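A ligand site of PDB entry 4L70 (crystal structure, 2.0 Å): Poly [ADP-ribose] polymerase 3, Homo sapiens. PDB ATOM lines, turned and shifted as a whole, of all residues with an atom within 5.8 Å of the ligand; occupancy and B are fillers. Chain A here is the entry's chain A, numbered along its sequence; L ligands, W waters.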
ATOM      1  N   ASP A 109      20.574 -34.867 -21.127  1.00  0.00           N
ATOM      2  CA  ASP A 109      20.474 -33.554 -21.754  1.00  0.00           C
ATOM      3  C   ASP A 109      19.038 -33.060 -21.988  1.00  0.00           C
ATOM      4  O   ASP A 109      18.724 -31.902 -21.690  1.00  0.00           O
ATOM      5  CB  ASP A 109      21.287 -33.515 -23.057  1.00  0.00           C
ATOM      6  CG  ASP A 109      22.796 -33.552 -22.810  1.00  0.00           C
ATOM      7  OD1 ASP A 109      23.224 -33.502 -21.628  1.00  0.00           O
ATOM      8  OD2 ASP A 109      23.572 -33.635 -23.793  1.00  0.00           O
ATOM      9  N   LEU A 112      17.799 -32.114 -18.601  1.00  0.00           N
ATOM     10  CA  LEU A 112      18.371 -30.799 -18.183  1.00  0.00           C
ATOM     11  C   LEU A 112      17.616 -29.603 -18.800  1.00  0.00           C
ATOM     12  O   LEU A 112      17.355 -28.549 -18.119  1.00  0.00           O
ATOM     13  CB  LEU A 112      19.861 -30.700 -18.496  1.00  0.00           C
ATOM     14  CG  LEU A 112      20.840 -31.546 -17.649  1.00  0.00           C
ATOM     15  CD1 LEU A 112      22.209 -31.648 -18.270  1.00  0.00           C
ATOM     16  CD2 LEU A 112      20.885 -31.012 -16.215  1.00  0.00           C
ATOM     17  N   VAL A 113      17.283 -29.744 -20.078  1.00  0.00           N
ATOM     18  CA  VAL A 113      16.437 -28.757 -20.765  1.00  0.00           C
ATOM     19  C   VAL A 113      15.064 -28.715 -20.088  1.00  0.00           C
ATOM     20  O   VAL A 113      14.581 -27.661 -19.760  1.00  0.00           O
ATOM     21  CB  VAL A 113      16.295 -29.059 -22.284  1.00  0.00           C
ATOM     22  CG1 VAL A 113      15.270 -28.091 -22.959  1.00  0.00           C
ATOM     23  CG2 VAL A 113      17.647 -28.973 -23.010  1.00  0.00           C
ATOM     24  N   ASP A 116      14.957 -26.801 -16.899  1.00  0.00           N
ATOM     25  CA  ASP A 116      14.951 -25.365 -17.057  1.00  0.00           C
ATOM     26  C   ASP A 116      13.612 -24.835 -17.564  1.00  0.00           C
ATOM     27  O   ASP A 116      13.263 -23.687 -17.302  1.00  0.00           O
ATOM     28  CB  ASP A 116      16.090 -24.916 -18.020  1.00  0.00           C
ATOM     29  CG  ASP A 116      17.438 -24.803 -17.310  1.00  0.00           C
ATOM     30  OD1 ASP A 116      17.532 -25.124 -16.059  1.00  0.00           O
ATOM     31  OD2 ASP A 116      18.401 -24.385 -17.990  1.00  0.00           O
ATOM     32  N   TRP A 208      31.528 -17.557 -27.193  1.00  0.00           N
ATOM     33  CA  TRP A 208      30.152 -17.867 -27.553  1.00  0.00           C
ATOM     34  C   TRP A 208      29.628 -18.997 -26.724  1.00  0.00           C
ATOM     35  O   TRP A 208      30.372 -19.940 -26.409  1.00  0.00           O
ATOM     36  CB  TRP A 208      30.051 -18.296 -29.014  1.00  0.00           C
ATOM     37  CG  TRP A 208      30.482 -17.196 -29.964  1.00  0.00           C
ATOM     38  CD1 TRP A 208      31.679 -17.068 -30.592  1.00  0.00           C
ATOM     39  CD2 TRP A 208      29.717 -16.047 -30.323  1.00  0.00           C
ATOM     40  NE1 TRP A 208      31.683 -15.946 -31.387  1.00  0.00           N
ATOM     41  CE2 TRP A 208      30.504 -15.269 -31.200  1.00  0.00           C
ATOM     42  CE3 TRP A 208      28.433 -15.618 -30.013  1.00  0.00           C
ATOM     43  CZ2 TRP A 208      30.059 -14.090 -31.766  1.00  0.00           C
ATOM     44  CZ3 TRP A 208      27.988 -14.429 -30.569  1.00  0.00           C
ATOM     45  CH2 TRP A 208      28.782 -13.684 -31.435  1.00  0.00           C
ATOM     46  N   HIS A 209      28.344 -18.907 -26.370  1.00  0.00           N
ATOM     47  CA  HIS A 209      27.607 -20.020 -25.813  1.00  0.00           C
ATOM     48  C   HIS A 209      26.205 -20.026 -26.502  1.00  0.00           C
ATOM     49  O   HIS A 209      25.405 -19.119 -26.324  1.00  0.00           O
ATOM     50  CB  HIS A 209      27.500 -19.884 -24.295  1.00  0.00           C
ATOM     51  CG  HIS A 209      26.838 -21.065 -23.622  1.00  0.00           C
ATOM     52  ND1 HIS A 209      27.535 -22.192 -23.278  1.00  0.00           N
ATOM     53  CD2 HIS A 209      25.557 -21.267 -23.218  1.00  0.00           C
ATOM     54  CE1 HIS A 209      26.708 -23.063 -22.718  1.00  0.00           C
ATOM     55  NE2 HIS A 209      25.488 -22.542 -22.693  1.00  0.00           N
ATOM     56  N   GLY A 210      25.958 -21.012 -27.376  1.00  0.00           N
ATOM     57  CA  GLY A 210      24.651 -21.101 -28.034  1.00  0.00           C
ATOM     58  C   GLY A 210      23.781 -22.070 -27.263  1.00  0.00           C
ATOM     59  O   GLY A 210      24.307 -23.062 -26.772  1.00  0.00           O
ATOM     60  N   THR A 211      22.484 -21.853 -27.152  1.00  0.00           N
ATOM     61  CA  THR A 211      21.537 -22.773 -26.518  1.00  0.00           C
ATOM     62  C   THR A 211      20.109 -22.837 -27.142  1.00  0.00           C
ATOM     63  O   THR A 211      19.816 -22.097 -27.957  1.00  0.00           O
ATOM     64  CB  THR A 211      21.265 -22.455 -25.024  1.00  0.00           C
ATOM     65  OG1 THR A 211      20.482 -21.293 -24.930  1.00  0.00           O
ATOM     66  CG2 THR A 211      22.501 -22.271 -24.217  1.00  0.00           C
ATOM     67  N   ASN A 212      19.295 -23.754 -26.656  1.00  0.00           N
ATOM     68  CA  ASN A 212      17.866 -23.832 -26.851  1.00  0.00           C
ATOM     69  C   ASN A 212      17.220 -22.526 -26.368  1.00  0.00           C
ATOM     70  O   ASN A 212      17.522 -22.052 -25.331  1.00  0.00           O
ATOM     71  CB  ASN A 212      17.283 -24.913 -25.929  1.00  0.00           C
ATOM     72  CG  ASN A 212      17.193 -26.257 -26.566  1.00  0.00           C
ATOM     73  OD1 ASN A 212      16.201 -26.609 -27.117  1.00  0.00           O
ATOM     74  ND2 ASN A 212      18.223 -27.022 -26.419  1.00  0.00           N
ATOM     75  N   VAL A 215      15.919 -22.537 -22.685  1.00  0.00           N
ATOM     76  CA  VAL A 215      16.721 -22.410 -21.466  1.00  0.00           C
ATOM     77  C   VAL A 215      17.216 -20.974 -21.242  1.00  0.00           C
ATOM     78  O   VAL A 215      17.911 -20.702 -20.247  1.00  0.00           O
ATOM     79  CB  VAL A 215      17.874 -23.455 -21.424  1.00  0.00           C
ATOM     80  CG1 VAL A 215      17.341 -24.867 -21.783  1.00  0.00           C
ATOM     81  CG2 VAL A 215      19.027 -23.042 -22.316  1.00  0.00           C
ATOM     82  N   ARG A 225      25.489 -22.764 -15.864  1.00  0.00           N
ATOM     83  CA  ARG A 225      25.577 -23.646 -14.699  1.00  0.00           C
ATOM     84  C   ARG A 225      26.176 -24.971 -15.113  1.00  0.00           C
ATOM     85  O   ARG A 225      26.136 -25.338 -16.297  1.00  0.00           O
ATOM     86  CB  ARG A 225      24.148 -23.886 -14.143  1.00  0.00           C
ATOM     87  CG  ARG A 225      23.557 -22.709 -13.350  1.00  0.00           C
ATOM     88  CD  ARG A 225      22.004 -22.643 -13.477  1.00  0.00           C
ATOM     89  NE  ARG A 225      21.651 -22.446 -14.895  1.00  0.00           N
ATOM     90  CZ  ARG A 225      20.609 -22.987 -15.527  1.00  0.00           C
ATOM     91  NH1 ARG A 225      19.693 -23.696 -14.869  1.00  0.00           N
ATOM     92  NH2 ARG A 225      20.472 -22.813 -16.841  1.00  0.00           N
ATOM     93  N   MET A 227      25.598 -28.829 -13.972  1.00  0.00           N
ATOM     94  CA  MET A 227      24.629 -29.645 -13.221  1.00  0.00           C
ATOM     95  C   MET A 227      25.206 -31.048 -13.056  1.00  0.00           C
ATOM     96  O   MET A 227      26.108 -31.465 -13.815  1.00  0.00           O
ATOM     97  CB  MET A 227      23.287 -29.623 -13.951  1.00  0.00           C
ATOM     98  CG  MET A 227      22.919 -28.215 -14.609  1.00  0.00           C
ATOM     99  SD  MET A 227      22.223 -27.005 -13.472  1.00  0.00           S
ATOM    100  CE  MET A 227      21.226 -28.085 -12.414  1.00  0.00           C
ATOM    101  N   SER A 230      25.527 -33.049 -16.238  1.00  0.00           N
ATOM    102  CA  SER A 230      26.190 -32.350 -17.372  1.00  0.00           C
ATOM    103  C   SER A 230      27.320 -33.224 -17.856  1.00  0.00           C
ATOM    104  O   SER A 230      28.004 -33.793 -17.063  1.00  0.00           O
ATOM    105  CB  SER A 230      26.882 -31.061 -16.899  1.00  0.00           C
ATOM    106  OG  SER A 230      25.979 -30.084 -16.517  1.00  0.00           O
ATOM    107  N   TYR A 239      30.603 -25.224 -21.538  1.00  0.00           N
ATOM    108  CA  TYR A 239      31.204 -25.243 -22.850  1.00  0.00           C
ATOM    109  C   TYR A 239      30.986 -23.927 -23.587  1.00  0.00           C
ATOM    110  O   TYR A 239      29.867 -23.430 -23.672  1.00  0.00           O
ATOM    111  CB  TYR A 239      30.513 -26.344 -23.720  1.00  0.00           C
ATOM    112  CG  TYR A 239      30.845 -27.775 -23.290  1.00  0.00           C
ATOM    113  CD1 TYR A 239      31.737 -28.534 -24.040  1.00  0.00           C
ATOM    114  CD2 TYR A 239      30.245 -28.362 -22.197  1.00  0.00           C
ATOM    115  CE1 TYR A 239      32.061 -29.803 -23.711  1.00  0.00           C
ATOM    116  CE2 TYR A 239      30.589 -29.674 -21.802  1.00  0.00           C
ATOM    117  CZ  TYR A 239      31.500 -30.384 -22.569  1.00  0.00           C
ATOM    118  OH  TYR A 239      31.917 -31.671 -22.259  1.00  0.00           O
ATOM    119  N   PHE A 240      32.069 -23.418 -24.147  1.00  0.00           N
ATOM    120  CA  PHE A 240      32.071 -22.260 -24.995  1.00  0.00           C
ATOM    121  C   PHE A 240      32.818 -22.559 -26.288  1.00  0.00           C
ATOM    122  O   PHE A 240      33.570 -23.503 -26.371  1.00  0.00           O
ATOM    123  CB  PHE A 240      32.758 -21.092 -24.293  1.00  0.00           C
ATOM    124  CG  PHE A 240      32.174 -20.728 -22.984  1.00  0.00           C
ATOM    125  CD1 PHE A 240      31.242 -19.737 -22.894  1.00  0.00           C
ATOM    126  CD2 PHE A 240      32.569 -21.371 -21.812  1.00  0.00           C
ATOM    127  CE1 PHE A 240      30.691 -19.371 -21.677  1.00  0.00           C
ATOM    128  CE2 PHE A 240      32.037 -21.021 -20.591  1.00  0.00           C
ATOM    129  CZ  PHE A 240      31.107 -19.986 -20.513  1.00  0.00           C
ATOM    130  N   ALA A 241      32.629 -21.717 -27.273  1.00  0.00           N
ATOM    131  CA  ALA A 241      33.412 -21.759 -28.508  1.00  0.00           C
ATOM    132  C   ALA A 241      33.939 -20.375 -28.848  1.00  0.00           C
ATOM    133  O   ALA A 241      33.287 -19.327 -28.579  1.00  0.00           O
ATOM    134  CB  ALA A 241      32.532 -22.263 -29.613  1.00  0.00           C
ATOM    135  N   LYS A 246      30.487 -22.901 -34.402  1.00  0.00           N
ATOM    136  CA  LYS A 246      30.400 -24.055 -33.504  1.00  0.00           C
ATOM    137  C   LYS A 246      29.239 -23.929 -32.495  1.00  0.00           C
ATOM    138  O   LYS A 246      28.410 -24.838 -32.316  1.00  0.00           O
ATOM    139  CB  LYS A 246      31.740 -24.237 -32.780  1.00  0.00           C
ATOM    140  CG  LYS A 246      31.778 -25.353 -31.772  1.00  0.00           C
ATOM    141  CD  LYS A 246      31.764 -26.689 -32.421  1.00  0.00           C
ATOM    142  CE  LYS A 246      31.803 -27.822 -31.387  1.00  0.00           C
ATOM    143  NZ  LYS A 246      31.218 -29.084 -31.990  1.00  0.00           N
ATOM    144  N   SER A 247      29.178 -22.796 -31.785  1.00  0.00           N
ATOM    145  CA  SER A 247      28.065 -22.522 -30.888  1.00  0.00           C
ATOM    146  C   SER A 247      26.696 -22.464 -31.572  1.00  0.00           C
ATOM    147  O   SER A 247      25.717 -22.875 -30.994  1.00  0.00           O
ATOM    148  CB  SER A 247      28.313 -21.225 -30.131  1.00  0.00           C
ATOM    149  OG  SER A 247      29.320 -21.441 -29.148  1.00  0.00           O
ATOM    150  N   ALA A 248      26.648 -21.974 -32.810  1.00  0.00           N
ATOM    151  CA  ALA A 248      25.356 -21.834 -33.518  1.00  0.00           C
ATOM    152  C   ALA A 248      24.711 -23.188 -33.808  1.00  0.00           C
ATOM    153  O   ALA A 248      23.472 -23.277 -33.909  1.00  0.00           O
ATOM    154  CB  ALA A 248      25.547 -21.040 -34.805  1.00  0.00           C
ATOM    155  N   TYR A 250      24.309 -25.431 -31.688  1.00  0.00           N
ATOM    156  CA  TYR A 250      23.527 -25.793 -30.521  1.00  0.00           C
ATOM    157  C   TYR A 250      22.314 -24.887 -30.342  1.00  0.00           C
ATOM    158  O   TYR A 250      21.575 -25.047 -29.395  1.00  0.00           O
ATOM    159  CB  TYR A 250      24.421 -25.802 -29.268  1.00  0.00           C
ATOM    160  CG  TYR A 250      25.582 -26.751 -29.375  1.00  0.00           C
ATOM    161  CD1 TYR A 250      25.453 -28.089 -29.009  1.00  0.00           C
ATOM    162  CD2 TYR A 250      26.780 -26.331 -29.890  1.00  0.00           C
ATOM    163  CE1 TYR A 250      26.527 -28.998 -29.118  1.00  0.00           C
ATOM    164  CE2 TYR A 250      27.881 -27.218 -30.011  1.00  0.00           C
ATOM    165  CZ  TYR A 250      27.745 -28.538 -29.613  1.00  0.00           C
ATOM    166  OH  TYR A 250      28.809 -29.363 -29.740  1.00  0.00           O
ATOM    167  N   SER A 338      37.468 -25.535 -31.700  1.00  0.00           N
ATOM    168  CA  SER A 338      37.841 -25.561 -30.288  1.00  0.00           C
ATOM    169  C   SER A 338      36.629 -25.530 -29.380  1.00  0.00           C
ATOM    170  O   SER A 338      35.635 -24.830 -29.702  1.00  0.00           O
ATOM    171  CB  SER A 338      38.750 -24.380 -29.933  1.00  0.00           C
ATOM    172  OG  SER A 338      39.999 -24.498 -30.550  1.00  0.00           O
ATOM    173  N   GLU A 339      36.692 -26.281 -28.278  1.00  0.00           N
ATOM    174  CA  GLU A 339      35.719 -26.212 -27.180  1.00  0.00           C
ATOM    175  C   GLU A 339      36.460 -25.755 -25.945  1.00  0.00           C
ATOM    176  O   GLU A 339      37.460 -26.378 -25.540  1.00  0.00           O
ATOM    177  CB  GLU A 339      35.039 -27.553 -26.947  1.00  0.00           C
ATOM    178  CG  GLU A 339      34.457 -28.130 -28.256  1.00  0.00           C
ATOM    179  CD  GLU A 339      33.578 -29.335 -28.078  1.00  0.00           C
ATOM    180  OE1 GLU A 339      33.195 -29.675 -26.940  1.00  0.00           O
ATOM    181  OE2 GLU A 339      33.292 -29.985 -29.117  1.00  0.00           O
ATOM    182  N   TYR A 340      35.988 -24.653 -25.371  1.00  0.00           N
ATOM    183  CA  TYR A 340      36.580 -24.030 -24.203  1.00  0.00           C
ATOM    184  C   TYR A 340      35.750 -24.383 -22.982  1.00  0.00           C
ATOM    185  O   TYR A 340      34.576 -24.064 -22.946  1.00  0.00           O
ATOM    186  CB  TYR A 340      36.580 -22.511 -24.331  1.00  0.00           C
ATOM    187  CG  TYR A 340      37.561 -21.903 -25.296  1.00  0.00           C
ATOM    188  CD1 TYR A 340      38.607 -21.141 -24.831  1.00  0.00           C
ATOM    189  CD2 TYR A 340      37.448 -22.099 -26.693  1.00  0.00           C
ATOM    190  CE1 TYR A 340      39.514 -20.564 -25.704  1.00  0.00           C
ATOM    191  CE2 TYR A 340      38.339 -21.526 -27.561  1.00  0.00           C
ATOM    192  CZ  TYR A 340      39.366 -20.772 -27.067  1.00  0.00           C
ATOM    193  OH  TYR A 340      40.275 -20.206 -27.920  1.00  0.00           O
HETATM  194  C1  LIG L   1      22.726 -27.829 -19.902  1.00  0.00           C
HETATM  195  C2  LIG L   1      22.432 -27.559 -18.555  1.00  0.00           C
HETATM  196  C3  LIG L   1      21.189 -27.012 -18.213  1.00  0.00           C
HETATM  197  C4  LIG L   1      20.282 -26.756 -19.241  1.00  0.00           C
HETATM  198  C5  LIG L   1      20.571 -27.000 -20.563  1.00  0.00           C
HETATM  199  C6  LIG L   1      21.786 -27.552 -20.918  1.00  0.00           C
HETATM  200  C7  LIG L   1      22.048 -27.803 -22.270  1.00  0.00           C
HETATM  201  C8  LIG L   1      21.832 -29.288 -22.487  1.00  0.00           C
HETATM  202  C9  LIG L   1      21.616 -29.447 -23.998  1.00  0.00           C
HETATM  203  N1  LIG L   1      23.407 -27.319 -22.681  1.00  0.00           N
HETATM  204  C10 LIG L   1      23.554 -26.293 -23.561  1.00  0.00           C
HETATM  205  O1  LIG L   1      22.605 -25.683 -24.054  1.00  0.00           O
HETATM  206  C11 LIG L   1      24.989 -25.895 -23.964  1.00  0.00           C
HETATM  207  C12 LIG L   1      25.129 -26.285 -25.441  1.00  0.00           C
HETATM  208  C13 LIG L   1      26.364 -25.891 -26.001  1.00  0.00           C
HETATM  209  N2  LIG L   1      27.353 -26.782 -26.101  1.00  0.00           N
HETATM  210  C14 LIG L   1      28.550 -26.446 -26.615  1.00  0.00           C
HETATM  211  C15 LIG L   1      29.482 -27.458 -26.743  1.00  0.00           C
HETATM  212  C16 LIG L   1      30.754 -27.163 -27.291  1.00  0.00           C
HETATM  213  C17 LIG L   1      31.007 -25.866 -27.734  1.00  0.00           C
HETATM  214  C18 LIG L   1      30.024 -24.856 -27.610  1.00  0.00           C
HETATM  215  C19 LIG L   1      28.797 -25.154 -27.081  1.00  0.00           C
HETATM  216  C20 LIG L   1      27.793 -24.157 -26.992  1.00  0.00           C
HETATM  217  O2  LIG L   1      27.931 -22.971 -27.381  1.00  0.00           O
HETATM  218  N3  LIG L   1      26.567 -24.587 -26.438  1.00  0.00           N
HETATM  219  O   HOH W   1      26.123 -28.832 -22.071  1.00  0.00           O
HETATM  220  O   HOH W   2      26.748 -29.080 -24.846  1.00  0.00           O
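ND1 of His 209 is in hydrogen-bond range of O of Tyr 239. The side-chain carboxylate (OE2) of Glu 339 is in salt-bridge range of the side-chain amino group (NZ) of Lys 246. The side-chain carboxylate (OD2) of Asp 116 lies within salt-bridge range of the guanidinium group (NH2) of Arg 225 (2.8 Å). O of Tyr 340 sits at hydrogen-bond distance from N of Phe 240, at 2.9 Å. NZ of Lys 246 lies within hydrogen-bond range of OH of Tyr 250, at 3.3 Å. OG of Ser 247 lies close to O of Trp 208 (3.3 Å).
OG of Ser 247 lies within hydrogen-bond range of O2 of the ligand, 2.7 Å away. The backbone NH of Gly 210 is in hydrogen-bond range of an oxygen (O2) of the ligand (2.8 Å). O of Gly 210 sits at hydrogen-bond distance from N3 of the ligand, at 2.7 Å.
Leu 112 touches the ligand. Asp 116 touches the ligand (OD2 to C4, 3.3 Å). His 209 touches the ligand. CG2 of Thr 211 touches O1 of the ligand, 3.4 Å away. Tyr 239 touches the ligand. Phe 240 touches the ligand. Tyr 250 touches the ligand. Glu 339 touches the ligand. Hydrophobic or aromatic side chains that line the ligand: Leu 112, His 209, Tyr 239 and Tyr 250. Of the 23 residues printed, 10 come within 4 Å of the ligand. The nearest printed residue that does not touch the ligand is Trp 208 (4.01 Å).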
